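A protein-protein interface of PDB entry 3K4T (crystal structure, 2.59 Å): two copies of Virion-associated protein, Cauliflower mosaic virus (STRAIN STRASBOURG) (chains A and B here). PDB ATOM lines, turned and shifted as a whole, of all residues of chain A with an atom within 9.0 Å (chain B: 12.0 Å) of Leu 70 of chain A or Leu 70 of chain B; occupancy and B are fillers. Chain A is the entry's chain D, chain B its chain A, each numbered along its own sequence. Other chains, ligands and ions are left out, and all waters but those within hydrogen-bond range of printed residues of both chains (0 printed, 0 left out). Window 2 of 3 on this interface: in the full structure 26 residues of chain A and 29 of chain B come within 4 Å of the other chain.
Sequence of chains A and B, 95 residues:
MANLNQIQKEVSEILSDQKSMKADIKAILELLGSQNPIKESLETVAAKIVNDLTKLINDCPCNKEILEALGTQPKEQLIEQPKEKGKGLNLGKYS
Of the 8 printed residues of chain A, 4 touch a printed residue of chain B.
Of the 10 printed residues of chain B, 4 touch a printed residue of chain A.
Hydrophobic or aromatic side chains of chain B within 4 Å of the printed part of chain A: Ile 66, Leu 67 and Leu 70.
Along chain B the printed residues that touch a printed residue of chain A span positions 63 to 70.
Among the printed residues, no Asp or Glu carboxylate lies within 4 Å of a Lys or Arg side-chain nitrogen of the other chain.
Among the printed residues, pairs that only touch across the chains: Ile 66 of chain A with Leu 67 of chain B (3.5 Å), Ile 66 of chain A with Asn 63 of chain B (3.7 Å), Ile 66 of chain A with Ile 66 of chain B (3.7 Å), Glu 65 of chain A with Leu 67 of chain B (3.7 Å), Leu 70 of chain A with Leu 70 of chain B (3.8 Å) and Ala 69 of chain A with Leu 70 of chain B (3.9 Å).
Glu 65 of chain A touches Asn 63 of chain B, but with the chains exchanged Asn 63 of chain A does not touch Glu 65 of chain B (12.4 Å).
Ile 66 of chain A touches Asn 63 of chain B, but with the chains exchanged Asn 63 of chain A does not touch Ile 66 of chain B (7.8 Å).
Ile 66 of chain A touches Leu 67 of chain B, but with the chains exchanged Leu 67 of chain A does not touch Ile 66 of chain B (7.7 Å).
Leu 70 of chain A touches its own counterpart, Leu 70 of chain B.
Positions printed for both chains: 63, 64, 65, 66, 67, 68, 69 and 70.
Leu 70 of chain A touches just one residue of chain B: Leu 70 (3.8 Å).
Printed residues of chain A within 4 Å of Leu 70 of chain B: Ala 69 and Leu 70.
Ala 69 of chain A touches one residue of chain B.
No residue of chain A comes within 4 Å of Ala 69 of chain B.
No residue of chain A comes within 4 Å of Gly 71 of chain B.
Of the printed residues of chain B, Ile 66 of chain A touches Asn 63 (3.7 Å), Ile 66 (3.7 Å) and Leu 67 (3.5 Å).
Of the printed residues of chain A, Asn 63 of chain B touches Glu 65 (3.0 Å) and Ile 66 (3.7 Å).
The nearest residue of chain B that does not touch Leu 70 of chain A is Ile 66 of chain B (7.0 Å).
The nearest printed residue of chain A that does not touch Leu 70 of chain B is Ile 66 of chain A (4.05 Å).
The side-chain carboxylate (OE1) of Glu 65 of chain A lies within hydrogen-bond range of the side-chain amide nitrogen (ND2) of Asn 63 of chain B (3.0 Å).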
ATOM      1  N   ASN A  63      11.051 -28.725 -15.423  1.00  0.00           N
ATOM      2  CA  ASN A  63      11.673 -28.808 -14.102  1.00  0.00           C
ATOM      3  C   ASN A  63      13.181 -29.075 -14.123  1.00  0.00           C
ATOM      4  O   ASN A  63      13.921 -28.505 -13.311  1.00  0.00           O
ATOM      5  CB  ASN A  63      10.947 -29.836 -13.232  1.00  0.00           C
ATOM      6  CG  ASN A  63       9.724 -29.259 -12.540  1.00  0.00           C
ATOM      7  OD1 ASN A  63       9.245 -28.176 -12.886  1.00  0.00           O
ATOM      8  ND2 ASN A  63       9.220 -29.978 -11.546  1.00  0.00           N
ATOM      9  N   LYS A  64      13.612 -29.946 -15.045  1.00  0.00           N
ATOM     10  CA  LYS A  64      15.033 -30.264 -15.319  1.00  0.00           C
ATOM     11  C   LYS A  64      16.031 -29.088 -15.376  1.00  0.00           C
ATOM     12  O   LYS A  64      17.154 -29.191 -14.882  1.00  0.00           O
ATOM     13  CB  LYS A  64      15.134 -30.980 -16.679  1.00  0.00           C
ATOM     14  CG  LYS A  64      16.514 -31.040 -17.339  1.00  0.00           C
ATOM     15  CD  LYS A  64      16.353 -31.005 -18.856  1.00  0.00           C
ATOM     16  CE  LYS A  64      17.684 -31.041 -19.588  1.00  0.00           C
ATOM     17  NZ  LYS A  64      18.203 -32.426 -19.729  1.00  0.00           N
ATOM     18  N   GLU A  65      15.599 -27.981 -15.971  1.00  0.00           N
ATOM     19  CA  GLU A  65      16.427 -26.792 -16.167  1.00  0.00           C
ATOM     20  C   GLU A  65      16.457 -25.942 -14.893  1.00  0.00           C
ATOM     21  O   GLU A  65      17.469 -25.296 -14.600  1.00  0.00           O
ATOM     22  CB  GLU A  65      15.894 -25.972 -17.340  1.00  0.00           C
ATOM     23  CG  GLU A  65      16.911 -25.093 -18.026  1.00  0.00           C
ATOM     24  CD  GLU A  65      16.624 -24.950 -19.508  1.00  0.00           C
ATOM     25  OE1 GLU A  65      15.439 -25.098 -19.898  1.00  0.00           O
ATOM     26  OE2 GLU A  65      17.578 -24.704 -20.284  1.00  0.00           O
ATOM     27  N   ILE A  66      15.344 -25.938 -14.156  1.00  0.00           N
ATOM     28  CA  ILE A  66      15.244 -25.214 -12.887  1.00  0.00           C
ATOM     29  C   ILE A  66      16.011 -25.936 -11.784  1.00  0.00           C
ATOM     30  O   ILE A  66      16.827 -25.330 -11.101  1.00  0.00           O
ATOM     31  CB  ILE A  66      13.759 -24.974 -12.482  1.00  0.00           C
ATOM     32  CG1 ILE A  66      13.115 -23.911 -13.393  1.00  0.00           C
ATOM     33  CG2 ILE A  66      13.606 -24.643 -10.976  1.00  0.00           C
ATOM     34  CD1 ILE A  66      13.999 -22.705 -13.693  1.00  0.00           C
ATOM     35  N   LEU A  67      15.763 -27.235 -11.630  1.00  0.00           N
ATOM     36  CA  LEU A  67      16.474 -28.051 -10.631  1.00  0.00           C
ATOM     37  C   LEU A  67      17.996 -28.064 -10.852  1.00  0.00           C
ATOM     38  O   LEU A  67      18.756 -28.298  -9.909  1.00  0.00           O
ATOM     39  CB  LEU A  67      15.976 -29.502 -10.643  1.00  0.00           C
ATOM     40  CG  LEU A  67      14.518 -29.904 -10.453  1.00  0.00           C
ATOM     41  CD1 LEU A  67      14.436 -31.415 -10.465  1.00  0.00           C
ATOM     42  CD2 LEU A  67      13.982 -29.357  -9.162  1.00  0.00           C
ATOM     43  N   GLU A  68      18.428 -27.838 -12.095  1.00  0.00           N
ATOM     44  CA  GLU A  68      19.855 -27.829 -12.445  1.00  0.00           C
ATOM     45  C   GLU A  68      20.550 -26.590 -11.903  1.00  0.00           C
ATOM     46  O   GLU A  68      21.771 -26.590 -11.739  1.00  0.00           O
ATOM     47  CB  GLU A  68      20.074 -27.906 -13.965  1.00  0.00           C
ATOM     48  CG  GLU A  68      20.061 -29.310 -14.560  1.00  0.00           C
ATOM     49  CD  GLU A  68      20.231 -29.314 -16.080  1.00  0.00           C
ATOM     50  OE1 GLU A  68      19.362 -29.879 -16.784  1.00  0.00           O
ATOM     51  OE2 GLU A  68      21.234 -28.750 -16.575  1.00  0.00           O
ATOM     52  N   ALA A  69      19.771 -25.540 -11.647  1.00  0.00           N
ATOM     53  CA  ALA A  69      20.301 -24.299 -11.095  1.00  0.00           C
ATOM     54  C   ALA A  69      20.264 -24.286  -9.561  1.00  0.00           C
ATOM     55  O   ALA A  69      20.873 -23.421  -8.936  1.00  0.00           O
ATOM     56  CB  ALA A  69      19.553 -23.107 -11.667  1.00  0.00           C
ATOM     57  N   LEU A  70      19.574 -25.261  -8.971  1.00  0.00           N
ATOM     58  CA  LEU A  70      19.371 -25.338  -7.524  1.00  0.00           C
ATOM     59  C   LEU A  70      20.312 -26.327  -6.845  1.00  0.00           C
ATOM     60  O   LEU A  70      21.512 -26.335  -7.105  1.00  0.00           O
ATOM     61  CB  LEU A  70      17.923 -25.727  -7.223  1.00  0.00           C
ATOM     62  CG  LEU A  70      16.807 -24.777  -7.668  1.00  0.00           C
ATOM     63  CD1 LEU A  70      15.486 -25.484  -7.623  1.00  0.00           C
ATOM     64  CD2 LEU A  70      16.757 -23.547  -6.789  1.00  0.00           C
ATOM     65  N   CYS B  62       8.141 -20.500 -19.252  1.00  0.00           N
ATOM     66  CA  CYS B  62       8.193 -20.045 -17.853  1.00  0.00           C
ATOM     67  C   CYS B  62       9.550 -20.213 -17.153  1.00  0.00           C
ATOM     68  O   CYS B  62       9.750 -19.709 -16.049  1.00  0.00           O
ATOM     69  CB  CYS B  62       7.066 -20.701 -17.041  1.00  0.00           C
ATOM     70  SG  CYS B  62       5.411 -20.407 -17.746  1.00  0.00           S
ATOM     71  N   ASN B  63      10.483 -20.902 -17.801  1.00  0.00           N
ATOM     72  CA  ASN B  63      11.810 -21.095 -17.234  1.00  0.00           C
ATOM     73  C   ASN B  63      12.603 -19.809 -17.094  1.00  0.00           C
ATOM     74  O   ASN B  63      13.349 -19.661 -16.130  1.00  0.00           O
ATOM     75  CB  ASN B  63      12.609 -22.113 -18.041  1.00  0.00           C
ATOM     76  CG  ASN B  63      12.351 -23.545 -17.597  1.00  0.00           C
ATOM     77  OD1 ASN B  63      11.515 -23.813 -16.724  1.00  0.00           O
ATOM     78  ND2 ASN B  63      13.074 -24.478 -18.208  1.00  0.00           N
ATOM     79  N   LYS B  64      12.441 -18.882 -18.030  1.00  0.00           N
ATOM     80  CA  LYS B  64      13.233 -17.652 -18.042  1.00  0.00           C
ATOM     81  C   LYS B  64      13.254 -16.870 -16.721  1.00  0.00           C
ATOM     82  O   LYS B  64      14.300 -16.730 -16.089  1.00  0.00           O
ATOM     83  CB  LYS B  64      12.768 -16.736 -19.178  1.00  0.00           C
ATOM     84  CG  LYS B  64      13.744 -15.620 -19.513  1.00  0.00           C
ATOM     85  CD  LYS B  64      13.028 -14.423 -20.121  1.00  0.00           C
ATOM     86  CE  LYS B  64      14.016 -13.366 -20.585  1.00  0.00           C
ATOM     87  NZ  LYS B  64      13.345 -12.278 -21.349  1.00  0.00           N
ATOM     88  N   GLU B  65      12.095 -16.353 -16.325  1.00  0.00           N
ATOM     89  CA  GLU B  65      11.981 -15.403 -15.218  1.00  0.00           C
ATOM     90  C   GLU B  65      12.535 -15.989 -13.915  1.00  0.00           C
ATOM     91  O   GLU B  65      13.162 -15.282 -13.116  1.00  0.00           O
ATOM     92  CB  GLU B  65      10.527 -14.980 -15.032  1.00  0.00           C
ATOM     93  CG  GLU B  65      10.335 -13.804 -14.089  1.00  0.00           C
ATOM     94  CD  GLU B  65       8.876 -13.403 -13.955  1.00  0.00           C
ATOM     95  OE1 GLU B  65       8.017 -14.071 -14.568  1.00  0.00           O
ATOM     96  OE2 GLU B  65       8.595 -12.424 -13.226  1.00  0.00           O
ATOM     97  N   ILE B  66      12.295 -17.283 -13.727  1.00  0.00           N
ATOM     98  CA  ILE B  66      12.807 -18.055 -12.604  1.00  0.00           C
ATOM     99  C   ILE B  66      14.322 -18.227 -12.681  1.00  0.00           C
ATOM    100  O   ILE B  66      15.012 -18.087 -11.668  1.00  0.00           O
ATOM    101  CB  ILE B  66      12.095 -19.413 -12.508  1.00  0.00           C
ATOM    102  CG1 ILE B  66      10.587 -19.182 -12.380  1.00  0.00           C
ATOM    103  CG2 ILE B  66      12.627 -20.222 -11.317  1.00  0.00           C
ATOM    104  CD1 ILE B  66       9.755 -20.430 -12.463  1.00  0.00           C
ATOM    105  N   LEU B  67      14.847 -18.503 -13.878  1.00  0.00           N
ATOM    106  CA  LEU B  67      16.299 -18.516 -14.093  1.00  0.00           C
ATOM    107  C   LEU B  67      16.918 -17.120 -14.006  1.00  0.00           C
ATOM    108  O   LEU B  67      18.115 -16.993 -13.734  1.00  0.00           O
ATOM    109  CB  LEU B  67      16.663 -19.191 -15.409  1.00  0.00           C
ATOM    110  CG  LEU B  67      16.296 -20.668 -15.595  1.00  0.00           C
ATOM    111  CD1 LEU B  67      16.363 -21.043 -17.088  1.00  0.00           C
ATOM    112  CD2 LEU B  67      17.164 -21.591 -14.752  1.00  0.00           C
ATOM    113  N   GLU B  68      16.110 -16.076 -14.226  1.00  0.00           N
ATOM    114  CA  GLU B  68      16.524 -14.685 -13.941  1.00  0.00           C
ATOM    115  C   GLU B  68      16.796 -14.507 -12.458  1.00  0.00           C
ATOM    116  O   GLU B  68      17.854 -13.996 -12.084  1.00  0.00           O
ATOM    117  CB  GLU B  68      15.458 -13.663 -14.357  1.00  0.00           C
ATOM    118  CG  GLU B  68      15.384 -13.348 -15.839  1.00  0.00           C
ATOM    119  CD  GLU B  68      14.273 -12.354 -16.157  1.00  0.00           C
ATOM    120  OE1 GLU B  68      14.448 -11.155 -15.852  1.00  0.00           O
ATOM    121  OE2 GLU B  68      13.224 -12.765 -16.716  1.00  0.00           O
ATOM    122  N   ALA B  69      15.836 -14.938 -11.630  1.00  0.00           N
ATOM    123  CA  ALA B  69      15.958 -14.840 -10.170  1.00  0.00           C
ATOM    124  C   ALA B  69      16.998 -15.797  -9.586  1.00  0.00           C
ATOM    125  O   ALA B  69      17.714 -15.448  -8.641  1.00  0.00           O
ATOM    126  CB  ALA B  69      14.621 -15.031  -9.505  1.00  0.00           C
ATOM    127  N   LEU B  70      17.098 -16.995 -10.151  1.00  0.00           N
ATOM    128  CA  LEU B  70      18.148 -17.933  -9.736  1.00  0.00           C
ATOM    129  C   LEU B  70      19.549 -17.498 -10.239  1.00  0.00           C
ATOM    130  O   LEU B  70      20.575 -17.912  -9.689  1.00  0.00           O
ATOM    131  CB  LEU B  70      17.808 -19.374 -10.164  1.00  0.00           C
ATOM    132  CG  LEU B  70      16.598 -20.028  -9.497  1.00  0.00           C
ATOM    133  CD1 LEU B  70      16.413 -21.480  -9.921  1.00  0.00           C
ATOM    134  CD2 LEU B  70      16.703 -19.969  -7.999  1.00  0.00           C
ATOM    135  N   GLY B  71      19.579 -16.654 -11.272  1.00  0.00           N
ATOM    136  CA  GLY B  71      20.823 -16.112 -11.797  1.00  0.00           C
ATOM    137  C   GLY B  71      21.502 -17.065 -12.764  1.00  0.00           C
ATOM    138  O   GLY B  71      22.644 -17.471 -12.546  1.00  0.00           O
